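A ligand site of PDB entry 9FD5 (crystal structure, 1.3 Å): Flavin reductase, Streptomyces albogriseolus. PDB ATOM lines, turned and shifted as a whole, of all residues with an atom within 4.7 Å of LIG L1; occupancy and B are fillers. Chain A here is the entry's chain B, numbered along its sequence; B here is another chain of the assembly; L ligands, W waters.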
ATOM      1  N   TYR A  17     -25.034 -23.003 -11.861  1.00  0.00           N
ATOM      2  CA  TYR A  17     -24.330 -22.197 -12.831  1.00  0.00           C
ATOM      3  C   TYR A  17     -24.777 -20.737 -12.792  1.00  0.00           C
ATOM      4  O   TYR A  17     -23.944 -19.835 -12.855  1.00  0.00           O
ATOM      5  CB  TYR A  17     -24.522 -22.798 -14.213  1.00  0.00           C
ATOM      6  CG  TYR A  17     -23.920 -21.996 -15.305  1.00  0.00           C
ATOM      7  CD1 TYR A  17     -22.573 -22.041 -15.551  1.00  0.00           C
ATOM      8  CD2 TYR A  17     -24.710 -21.191 -16.112  1.00  0.00           C
ATOM      9  CE1 TYR A  17     -21.994 -21.296 -16.560  1.00  0.00           C
ATOM     10  CE2 TYR A  17     -24.140 -20.436 -17.116  1.00  0.00           C
ATOM     11  CZ  TYR A  17     -22.781 -20.511 -17.345  1.00  0.00           C
ATOM     12  OH  TYR A  17     -22.174 -19.766 -18.330  1.00  0.00           O
ATOM     13  N   ARG A  18     -26.095 -20.481 -12.704  1.00  0.00           N
ATOM     14  CA  ARG A  18     -26.568 -19.107 -12.558  1.00  0.00           C
ATOM     15  C   ARG A  18     -25.977 -18.459 -11.323  1.00  0.00           C
ATOM     16  O   ARG A  18     -25.535 -17.309 -11.371  1.00  0.00           O
ATOM     17  CB  ARG A  18     -28.100 -19.031 -12.482  1.00  0.00           C
ATOM     18  CG  ARG A  18     -28.861 -19.317 -13.745  1.00  0.00           C
ATOM     19  CD  ARG A  18     -30.367 -18.987 -13.523  1.00  0.00           C
ATOM     20  NE  ARG A  18     -31.193 -19.386 -14.659  1.00  0.00           N
ATOM     21  CZ  ARG A  18     -31.886 -18.562 -15.454  1.00  0.00           C
ATOM     22  NH1 ARG A  18     -31.898 -17.255 -15.270  1.00  0.00           N
ATOM     23  NH2 ARG A  18     -32.598 -19.077 -16.443  1.00  0.00           N
ATOM     24  N   MET A  21     -22.285 -17.505 -12.164  1.00  0.00           N
ATOM     25  CA  MET A  21     -22.133 -16.382 -13.081  1.00  0.00           C
ATOM     26  C   MET A  21     -22.691 -15.089 -12.536  1.00  0.00           C
ATOM     27  O   MET A  21     -22.205 -14.012 -12.912  1.00  0.00           O
ATOM     28  CB  MET A  21     -22.711 -16.716 -14.458  1.00  0.00           C
ATOM     29  CG  MET A  21     -22.059 -17.954 -15.110  1.00  0.00           C
ATOM     30  SD  MET A  21     -20.259 -17.944 -15.233  1.00  0.00           S
ATOM     31  CE  MET A  21     -20.015 -16.703 -16.479  1.00  0.00           C
ATOM     32  N   SER A  22     -23.667 -15.164 -11.653  1.00  0.00           N
ATOM     33  CA  SER A  22     -24.143 -13.955 -11.012  1.00  0.00           C
ATOM     34  C   SER A  22     -23.019 -13.232 -10.283  1.00  0.00           C
ATOM     35  O   SER A  22     -22.986 -11.999 -10.226  1.00  0.00           O
ATOM     36  CB  SER A  22     -25.259 -14.330 -10.053  1.00  0.00           C
ATOM     37  OG  SER A  22     -25.752 -13.197  -9.399  1.00  0.00           O
ATOM     38  N   SER A  46     -24.983  -8.044 -21.048  1.00  0.00           N
ATOM     39  CA  SER A  46     -23.822  -8.037 -20.164  1.00  0.00           C
ATOM     40  C   SER A  46     -22.722  -8.966 -20.650  1.00  0.00           C
ATOM     41  O   SER A  46     -21.678  -9.087 -19.984  1.00  0.00           O
ATOM     42  CB  SER A  46     -24.209  -8.360 -18.725  1.00  0.00           C
ATOM     43  OG  SER A  46     -24.785  -9.657 -18.709  1.00  0.00           O
ATOM     44  N   SER A  47     -22.893  -9.555 -21.824  1.00  0.00           N
ATOM     45  CA  SER A  47     -21.911 -10.502 -22.359  1.00  0.00           C
ATOM     46  C   SER A  47     -20.865  -9.874 -23.272  1.00  0.00           C
ATOM     47  O   SER A  47     -20.074 -10.586 -23.888  1.00  0.00           O
ATOM     48  CB  SER A  47     -22.623 -11.660 -23.054  1.00  0.00           C
ATOM     49  OG  SER A  47     -23.355 -11.161 -24.163  1.00  0.00           O
ATOM     50  N   CYS A  61     -22.969 -12.376 -26.726  1.00  0.00           N
ATOM     51  CA  CYS A  61     -23.728 -13.629 -26.808  1.00  0.00           C
ATOM     52  C   CYS A  61     -25.198 -13.265 -26.766  1.00  0.00           C
ATOM     53  O   CYS A  61     -25.654 -12.655 -25.783  1.00  0.00           O
ATOM     54  CB  CYS A  61     -23.378 -14.532 -25.630  1.00  0.00           C
ATOM     55  SG  CYS A  61     -21.673 -15.034 -25.634  1.00  0.00           S
ATOM     56  N   ARG A  63     -29.384 -14.404 -27.567  1.00  0.00           N
ATOM     57  CA  ARG A  63     -30.316 -15.514 -27.648  1.00  0.00           C
ATOM     58  C   ARG A  63     -30.785 -15.757 -29.080  1.00  0.00           C
ATOM     59  O   ARG A  63     -31.225 -14.829 -29.775  1.00  0.00           O
ATOM     60  CB  ARG A  63     -31.532 -15.242 -26.772  1.00  0.00           C
ATOM     61  CG  ARG A  63     -32.426 -16.456 -26.630  1.00  0.00           C
ATOM     62  CD  ARG A  63     -33.712 -16.108 -25.944  1.00  0.00           C
ATOM     63  NE  ARG A  63     -34.698 -15.538 -26.859  1.00  0.00           N
ATOM     64  CZ  ARG A  63     -35.223 -14.322 -26.775  1.00  0.00           C
ATOM     65  NH1 ARG A  63     -34.821 -13.461 -25.868  1.00  0.00           N
ATOM     66  NH2 ARG A  63     -36.229 -14.003 -27.579  1.00  0.00           N
ATOM     67  N   ASP A 137     -28.487 -22.527 -27.299  1.00  0.00           N
ATOM     68  CA  ASP A 137     -29.583 -21.704 -27.779  1.00  0.00           C
ATOM     69  C   ASP A 137     -29.178 -20.250 -27.958  1.00  0.00           C
ATOM     70  O   ASP A 137     -30.046 -19.365 -28.018  1.00  0.00           O
ATOM     71  CB  ASP A 137     -30.798 -21.811 -26.862  1.00  0.00           C
ATOM     72  CG  ASP A 137     -30.556 -21.253 -25.486  1.00  0.00           C
ATOM     73  OD1 ASP A 137     -29.381 -21.059 -25.118  1.00  0.00           O
ATOM     74  OD2 ASP A 137     -31.562 -21.009 -24.786  1.00  0.00           O
ATOM     75  N   HIS A 138     -27.878 -19.985 -28.037  1.00  0.00           N
ATOM     76  CA  HIS A 138     -27.349 -18.630 -28.210  1.00  0.00           C
ATOM     77  C   HIS A 138     -26.409 -18.593 -29.392  1.00  0.00           C
ATOM     78  O   HIS A 138     -25.951 -19.616 -29.913  1.00  0.00           O
ATOM     79  CB  HIS A 138     -26.653 -18.112 -26.945  1.00  0.00           C
ATOM     80  CG  HIS A 138     -27.609 -17.766 -25.853  1.00  0.00           C
ATOM     81  ND1 HIS A 138     -28.381 -18.709 -25.226  1.00  0.00           N
ATOM     82  CD2 HIS A 138     -27.971 -16.574 -25.325  1.00  0.00           C
ATOM     83  CE1 HIS A 138     -29.182 -18.119 -24.360  1.00  0.00           C
ATOM     84  NE2 HIS A 138     -28.942 -16.821 -24.391  1.00  0.00           N
ATOM     85  N   TYR A 158     -23.632  -4.425 -13.029  1.00  0.00           N
ATOM     86  CA  TYR A 158     -24.612  -5.422 -12.622  1.00  0.00           C
ATOM     87  C   TYR A 158     -23.853  -6.613 -12.065  1.00  0.00           C
ATOM     88  O   TYR A 158     -22.910  -7.111 -12.680  1.00  0.00           O
ATOM     89  CB  TYR A 158     -25.554  -5.846 -13.792  1.00  0.00           C
ATOM     90  CG  TYR A 158     -26.791  -6.588 -13.315  1.00  0.00           C
ATOM     91  CD1 TYR A 158     -27.901  -5.901 -12.879  1.00  0.00           C
ATOM     92  CD2 TYR A 158     -26.803  -7.974 -13.239  1.00  0.00           C
ATOM     93  CE1 TYR A 158     -29.013  -6.557 -12.475  1.00  0.00           C
ATOM     94  CE2 TYR A 158     -27.913  -8.651 -12.813  1.00  0.00           C
ATOM     95  CZ  TYR A 158     -29.012  -7.937 -12.422  1.00  0.00           C
ATOM     96  OH  TYR A 158     -30.132  -8.600 -11.949  1.00  0.00           O
ATOM     97  N   ARG A 161     -27.081 -10.040  -8.746  1.00  0.00           N
ATOM     98  CA  ARG A 161     -28.498  -9.816  -8.977  1.00  0.00           C
ATOM     99  C   ARG A 161     -28.934  -8.398  -8.614  1.00  0.00           C
ATOM    100  O   ARG A 161     -30.076  -8.182  -8.229  1.00  0.00           O
ATOM    101  CB  ARG A 161     -29.370 -10.906  -8.345  1.00  0.00           C
ATOM    102  CG  ARG A 161     -28.878 -12.307  -8.755  1.00  0.00           C
ATOM    103  CD  ARG A 161     -29.903 -13.402  -8.450  1.00  0.00           C
ATOM    104  NE  ARG A 161     -29.495 -14.691  -9.025  1.00  0.00           N
ATOM    105  CZ  ARG A 161     -28.828 -15.638  -8.385  1.00  0.00           C
ATOM    106  NH1 ARG A 161     -28.572 -15.558  -7.087  1.00  0.00           N
ATOM    107  NH2 ARG A 161     -28.443 -16.716  -9.056  1.00  0.00           N
ATOM    108  N   SER B  50     -20.878 -15.854 -20.026  1.00  0.00           N
ATOM    109  CA  SER B  50     -21.801 -16.965 -20.161  1.00  0.00           C
ATOM    110  C   SER B  50     -22.247 -17.125 -21.609  1.00  0.00           C
ATOM    111  O   SER B  50     -22.568 -16.140 -22.286  1.00  0.00           O
ATOM    112  CB  SER B  50     -23.030 -16.749 -19.281  1.00  0.00           C
ATOM    113  OG  SER B  50     -23.840 -17.904 -19.360  1.00  0.00           O
ATOM    114  N   ALA B  51     -22.258 -18.367 -22.085  1.00  0.00           N
ATOM    115  CA  ALA B  51     -22.688 -18.693 -23.439  1.00  0.00           C
ATOM    116  C   ALA B  51     -24.103 -19.244 -23.467  1.00  0.00           C
ATOM    117  O   ALA B  51     -24.924 -18.752 -24.235  1.00  0.00           O
ATOM    118  CB  ALA B  51     -21.716 -19.685 -24.076  1.00  0.00           C
ATOM    119  N   THR B  52     -24.405 -20.257 -22.654  1.00  0.00           N
ATOM    120  CA  THR B  52     -25.725 -20.868 -22.698  1.00  0.00           C
ATOM    121  C   THR B  52     -25.944 -21.637 -21.413  1.00  0.00           C
ATOM    122  O   THR B  52     -24.987 -21.985 -20.713  1.00  0.00           O
ATOM    123  CB  THR B  52     -25.889 -21.764 -23.943  1.00  0.00           C
ATOM    124  OG1 THR B  52     -27.229 -22.240 -24.034  1.00  0.00           O
ATOM    125  CG2 THR B  52     -24.969 -22.969 -23.899  1.00  0.00           C
ATOM    126  N   LEU B  53     -27.220 -21.915 -21.113  1.00  0.00           N
ATOM    127  CA  LEU B  53     -27.595 -22.756 -19.989  1.00  0.00           C
ATOM    128  C   LEU B  53     -27.827 -24.205 -20.353  1.00  0.00           C
ATOM    129  O   LEU B  53     -27.977 -25.019 -19.442  1.00  0.00           O
ATOM    130  CB  LEU B  53     -28.895 -22.266 -19.352  1.00  0.00           C
ATOM    131  CG  LEU B  53     -28.869 -20.875 -18.747  1.00  0.00           C
ATOM    132  CD1 LEU B  53     -30.229 -20.543 -18.151  1.00  0.00           C
ATOM    133  CD2 LEU B  53     -27.802 -20.762 -17.690  1.00  0.00           C
HETATM  134  P1  LIG L   1     -29.800 -15.109 -12.784  1.00  0.00           P
HETATM  135  O1  LIG L   1     -29.519 -15.941 -11.604  1.00  0.00           O
HETATM  136  O2  LIG L   1     -31.014 -15.326 -13.626  1.00  0.00           O
HETATM  137  O3  LIG L   1     -28.552 -15.141 -13.842  1.00  0.00           O
HETATM  138  C1  LIG L   1     -27.221 -15.143 -13.338  1.00  0.00           C
HETATM  139  C2  LIG L   1     -26.269 -15.181 -14.515  1.00  0.00           C
HETATM  140  O4  LIG L   1     -26.460 -16.468 -15.167  1.00  0.00           O
HETATM  141  C3  LIG L   1     -26.451 -14.131 -15.623  1.00  0.00           C
HETATM  142  O5  LIG L   1     -25.774 -12.949 -15.280  1.00  0.00           O
HETATM  143  C4  LIG L   1     -25.748 -14.864 -16.775  1.00  0.00           C
HETATM  144  O6  LIG L   1     -24.354 -14.766 -16.706  1.00  0.00           O
HETATM  145  C5  LIG L   1     -26.231 -16.290 -16.551  1.00  0.00           C
HETATM  146  N1  LIG L   1     -27.432 -16.611 -17.286  1.00  0.00           N
HETATM  147  C6  LIG L   1     -28.722 -16.419 -16.860  1.00  0.00           C
HETATM  148  N2  LIG L   1     -29.604 -16.785 -17.727  1.00  0.00           N
HETATM  149  C7  LIG L   1     -28.880 -17.166 -18.838  1.00  0.00           C
HETATM  150  C8  LIG L   1     -29.252 -17.691 -20.099  1.00  0.00           C
HETATM  151  N3  LIG L   1     -30.526 -17.851 -20.450  1.00  0.00           N
HETATM  152  N4  LIG L   1     -28.266 -18.005 -20.946  1.00  0.00           N
HETATM  153  C9  LIG L   1     -27.016 -17.837 -20.556  1.00  0.00           C
HETATM  154  N5  LIG L   1     -26.531 -17.415 -19.390  1.00  0.00           N
HETATM  155  C10 LIG L   1     -27.518 -17.085 -18.573  1.00  0.00           C
HETATM  156  N6  LIG L   1     -33.032 -14.121 -20.588  1.00  0.00           N
HETATM  157  C11 LIG L   1     -33.968 -14.815 -21.266  1.00  0.00           C
HETATM  158  O7  LIG L   1     -35.161 -14.742 -21.040  1.00  0.00           O
HETATM  159  N7  LIG L   1     -33.574 -15.652 -22.301  1.00  0.00           N
HETATM  160  C12 LIG L   1     -32.305 -15.854 -22.724  1.00  0.00           C
HETATM  161  O8  LIG L   1     -32.022 -16.608 -23.610  1.00  0.00           O
HETATM  162  C13 LIG L   1     -31.285 -15.068 -21.981  1.00  0.00           C
HETATM  163  N8  LIG L   1     -30.030 -15.192 -22.310  1.00  0.00           N
HETATM  164  C14 LIG L   1     -29.108 -14.545 -21.610  1.00  0.00           C
HETATM  165  C15 LIG L   1     -27.763 -14.691 -21.975  1.00  0.00           C
HETATM  166  C16 LIG L   1     -26.743 -14.066 -21.331  1.00  0.00           C
HETATM  167  C17 LIG L   1     -25.315 -14.270 -21.770  1.00  0.00           C
HETATM  168  C18 LIG L   1     -27.093 -13.243 -20.240  1.00  0.00           C
HETATM  169  C19 LIG L   1     -26.005 -12.519 -19.515  1.00  0.00           C
HETATM  170  C20 LIG L   1     -28.418 -13.099 -19.839  1.00  0.00           C
HETATM  171  C21 LIG L   1     -29.463 -13.741 -20.510  1.00  0.00           C
HETATM  172  N9  LIG L   1     -30.806 -13.593 -20.203  1.00  0.00           N
HETATM  173  C22 LIG L   1     -31.746 -14.262 -20.894  1.00  0.00           C
HETATM  174  C23 LIG L   1     -31.236 -12.782 -19.036  1.00  0.00           C
HETATM  175  C24 LIG L   1     -31.041 -13.670 -17.771  1.00  0.00           C
HETATM  176  O9  LIG L   1     -31.854 -14.828 -17.760  1.00  0.00           O
HETATM  177  C25 LIG L   1     -31.270 -12.880 -16.483  1.00  0.00           C
HETATM  178  O10 LIG L   1     -32.612 -12.461 -16.477  1.00  0.00           O
HETATM  179  C26 LIG L   1     -30.307 -11.655 -16.388  1.00  0.00           C
HETATM  180  O11 LIG L   1     -29.012 -12.119 -16.735  1.00  0.00           O
HETATM  181  C27 LIG L   1     -30.351 -11.111 -14.958  1.00  0.00           C
HETATM  182  O12 LIG L   1     -30.221 -12.229 -14.125  1.00  0.00           O
HETATM  183  P2  LIG L   1     -29.613 -12.153 -12.651  1.00  0.00           P
HETATM  184  O13 LIG L   1     -28.129 -12.015 -12.938  1.00  0.00           O
HETATM  185  O14 LIG L   1     -30.106 -11.160 -11.738  1.00  0.00           O
HETATM  186  O15 LIG L   1     -29.791 -13.662 -12.140  1.00  0.00           O
HETATM  187  P1  LG2 L   2     -37.360 -10.536 -27.976  1.00  0.00           P
HETATM  188  O1  LG2 L   2     -37.591 -11.622 -26.996  1.00  0.00           O
HETATM  189  O2  LG2 L   2     -37.376 -10.829 -29.446  1.00  0.00           O
HETATM  190  O3  LG2 L   2     -38.484  -9.425 -27.660  1.00  0.00           O
HETATM  191  C1  LG2 L   2     -39.031  -8.620 -28.676  1.00  0.00           C
HETATM  192  C2  LG2 L   2     -39.671  -7.425 -28.001  1.00  0.00           C
HETATM  193  O4  LG2 L   2     -40.827  -7.905 -27.286  1.00  0.00           O
HETATM  194  C3  LG2 L   2     -38.784  -6.759 -26.956  1.00  0.00           C
HETATM  195  O5  LG2 L   2     -38.095  -5.697 -27.561  1.00  0.00           O
HETATM  196  C4  LG2 L   2     -39.814  -6.284 -25.936  1.00  0.00           C
HETATM  197  O6  LG2 L   2     -40.340  -5.052 -26.353  1.00  0.00           O
HETATM  198  C5  LG2 L   2     -40.839  -7.409 -25.974  1.00  0.00           C
HETATM  199  N1  LG2 L   2     -40.576  -8.485 -25.035  1.00  0.00           N
HETATM  200  C6  LG2 L   2     -39.372  -8.872 -24.467  1.00  0.00           C
HETATM  201  N2  LG2 L   2     -39.483  -9.912 -23.665  1.00  0.00           N
HETATM  202  C7  LG2 L   2     -40.817 -10.207 -23.698  1.00  0.00           C
HETATM  203  C8  LG2 L   2     -41.585 -11.183 -23.043  1.00  0.00           C
HETATM  204  N3  LG2 L   2     -41.026 -12.075 -22.218  1.00  0.00           N
HETATM  205  N4  LG2 L   2     -42.897 -11.217 -23.293  1.00  0.00           N
HETATM  206  C9  LG2 L   2     -43.429 -10.320 -24.117  1.00  0.00           C
HETATM  207  N5  LG2 L   2     -42.816  -9.356 -24.783  1.00  0.00           N
HETATM  208  C10 LG2 L   2     -41.508  -9.346 -24.533  1.00  0.00           C
HETATM  209  N6  LG2 L   2     -29.820 -11.554 -23.172  1.00  0.00           N
HETATM  210  C11 LG2 L   2     -28.939 -12.053 -24.085  1.00  0.00           C
HETATM  211  O7  LG2 L   2     -29.277 -12.767 -25.035  1.00  0.00           O
HETATM  212  N7  LG2 L   2     -27.583 -11.779 -23.926  1.00  0.00           N
HETATM  213  C12 LG2 L   2     -27.035 -11.051 -22.915  1.00  0.00           C
HETATM  214  O8  LG2 L   2     -25.850 -10.817 -22.834  1.00  0.00           O
HETATM  215  C13 LG2 L   2     -28.005 -10.540 -21.951  1.00  0.00           C
HETATM  216  N8  LG2 L   2     -27.573  -9.849 -20.933  1.00  0.00           N
HETATM  217  C14 LG2 L   2     -28.499  -9.370 -20.060  1.00  0.00           C
HETATM  218  C15 LG2 L   2     -28.050  -8.627 -18.944  1.00  0.00           C
HETATM  219  C16 LG2 L   2     -28.890  -8.113 -18.012  1.00  0.00           C
HETATM  220  C17 LG2 L   2     -28.392  -7.322 -16.846  1.00  0.00           C
HETATM  221  C18 LG2 L   2     -30.291  -8.331 -18.158  1.00  0.00           C
HETATM  222  C19 LG2 L   2     -31.302  -7.785 -17.192  1.00  0.00           C
HETATM  223  C20 LG2 L   2     -30.741  -9.032 -19.239  1.00  0.00           C
HETATM  224  C21 LG2 L   2     -29.889  -9.569 -20.203  1.00  0.00           C
HETATM  225  N9  LG2 L   2     -30.295 -10.321 -21.288  1.00  0.00           N
HETATM  226  C22 LG2 L   2     -29.391 -10.839 -22.167  1.00  0.00           C
HETATM  227  C23 LG2 L   2     -31.705 -10.582 -21.593  1.00  0.00           C
HETATM  228  C24 LG2 L   2     -32.209  -9.623 -22.714  1.00  0.00           C
HETATM  229  O9  LG2 L   2     -31.961  -8.260 -22.428  1.00  0.00           O
HETATM  230  C25 LG2 L   2     -33.728  -9.768 -22.886  1.00  0.00           C
HETATM  231  O10 LG2 L   2     -33.997 -11.140 -23.136  1.00  0.00           O
HETATM  232  C26 LG2 L   2     -34.349  -8.884 -23.994  1.00  0.00           C
HETATM  233  O11 LG2 L   2     -35.766  -8.929 -23.812  1.00  0.00           O
HETATM  234  C27 LG2 L   2     -34.023  -9.355 -25.406  1.00  0.00           C
HETATM  235  O12 LG2 L   2     -34.652  -8.421 -26.304  1.00  0.00           O
HETATM  236  P2  LG2 L   2     -34.983  -8.701 -27.848  1.00  0.00           P
HETATM  237  O13 LG2 L   2     -35.865  -7.531 -28.240  1.00  0.00           O
HETATM  238  O14 LG2 L   2     -33.782  -8.986 -28.619  1.00  0.00           O
HETATM  239  O15 LG2 L   2     -35.895 -10.028 -27.686  1.00  0.00           O
HETATM  240  O   HOH W   1     -26.153 -11.209 -11.228  1.00  0.00           O
HETATM  241  O   HOH W   2     -32.614 -11.604 -10.807  1.00  0.00           O
HETATM  242  O   HOH W   3     -29.443 -20.653 -22.413  1.00  0.00           O
HETATM  243  O   HOH W   4     -34.188 -10.550 -16.727  1.00  0.00           O
HETATM  244  O   HOH W   5     -23.387 -11.952 -17.214  1.00  0.00           O
HETATM  245  O   HOH W   6     -31.385 -17.515 -10.607  1.00  0.00           O
HETATM  246  O   HOH W   7     -32.159 -19.240 -22.867  1.00  0.00           O
HETATM  247  O   HOH W   8     -22.618 -13.722 -18.678  1.00  0.00           O
HETATM  248  O   HOH W   9     -33.105 -17.710 -18.851  1.00  0.00           O
HETATM  249  O   HOH W  10     -35.754 -17.362 -23.230  1.00  0.00           O
HETATM  250  O   HOH W  11     -35.495 -11.782 -20.989  1.00  0.00           O
HETATM  251  O   HOH W  12     -26.831 -10.637 -16.097  1.00  0.00           O
HETATM  252  O   HOH W  13     -33.408 -13.543 -13.914  1.00  0.00           O
HETATM  253  O   HOH W  14     -32.309 -12.891 -24.554  1.00  0.00           O
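O of Cys 61 is in hydrogen-bond range of N7 of LG2 L2, 2.8 Å away.
The side-chain hydroxyl (OH) of Tyr 158 lies within hydrogen-bond range of an oxygen (O14) of LIG L1 (2.6 Å).
An oxygen (O8) of LG2 L2 sits close to the backbone NH of Ser 47 (3.4 Å).
N5 of LIG L1 sits at hydrogen-bond distance from OG of Ser 50 of chain B (2.7 Å).
The side-chain hydroxyl (OG) of Ser 47 sits at hydrogen-bond distance from an oxygen (O8) of LG2 L2.
The backbone NH of Arg 63 is in hydrogen-bond range of an oxygen (O7) of LG2 L2, at 3.0 Å.
NE2 of His 138 is in hydrogen-bond range of N8 of LIG L1 (2.9 Å).
O1 of LIG L1 is in salt-bridge range of NE of Arg 161 (2.9 Å).
N of Ser 46 is in hydrogen-bond range of N8 of LG2 L2, 3.2 Å away.
O2 of LIG L1 is in salt-bridge range of NH1 of Arg 18.
The guanidinium group (NH2) of Arg 63 is in salt-bridge range of an oxygen (O1) of LG2 L2, at 2.8 Å.
The backbone NH (N) of Cys 61 sits at hydrogen-bond distance from the side-chain hydroxyl (OG) of Ser 47.
OD1 of Asp 137 sits at hydrogen-bond distance from OG1 of Thr 52 of chain B, at 2.7 Å.
The side-chain hydroxyl (OG) of Ser 50 of chain B is in hydrogen-bond range of the side-chain hydroxyl (OH) of Tyr 17, at 2.7 Å.
The side-chain carboxylate (OD1) of Asp 137 is in hydrogen-bond range of a ring nitrogen (ND1) of His 138 (2.6 Å).
O of Ser 50 of chain B lies within hydrogen-bond range of SG of Cys 61 (3.6 Å).
The backbone NH of Arg 161 sits close to the side-chain hydroxyl of Ser 22 (3.5 Å).
Merely in contact with LIG L1: Met 21 (3.4 Å), Ser 22 (3.9 Å), Ser 46 (3.2 Å), Ser 47 (3.96 Å), Arg 63 (2.9 Å), Thr 52 of chain B (3.9 Å) and Leu 53 of chain B (3.5 Å).
Hydrophobic or aromatic side chains that line LIG L1: Met 21, His 138, Tyr 158 and Leu 53 of chain B.
12 residues have an atom within 4 Å of LIG L1: Arg 18, Met 21, Ser 22, Ser 46, Ser 47, Arg 63, His 138, Tyr 158, Arg 161, Ser 50 of chain B, Thr 52 of chain B and Leu 53 of chain B.
The nearest printed residue that does not touch LIG L1 is Cys 61 (4.3 Å).
Water W6 bridges an oxygen (O1) of LIG L1 (2.6 Å) and the guanidinium group of Arg 161 (3.4 Å).
Water W12 bridges O5 of LIG L1 (2.7 Å) and OG of Ser 46 (3.5 Å).
Water W1 lies within hydrogen-bond range of the side-chain hydroxyl of Ser 22, an oxygen (O13) of LIG L1 and the backbone NH of Arg 161.
Water W11 lies within hydrogen-bond range of O10 of LG2 L2 (2.7 Å) and O7 of LIG L1 (3.0 Å).
Water W5 bridges O6 of LIG L1 and OG of Ser 46.
Water W3 lies within hydrogen-bond range of OD1 of Asp 137 (2.7 Å), N of Leu 53 of chain B (2.9 Å), OG1 of Thr 52 of chain B (3.2 Å) and N4 of LIG L1 (3.2 Å).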
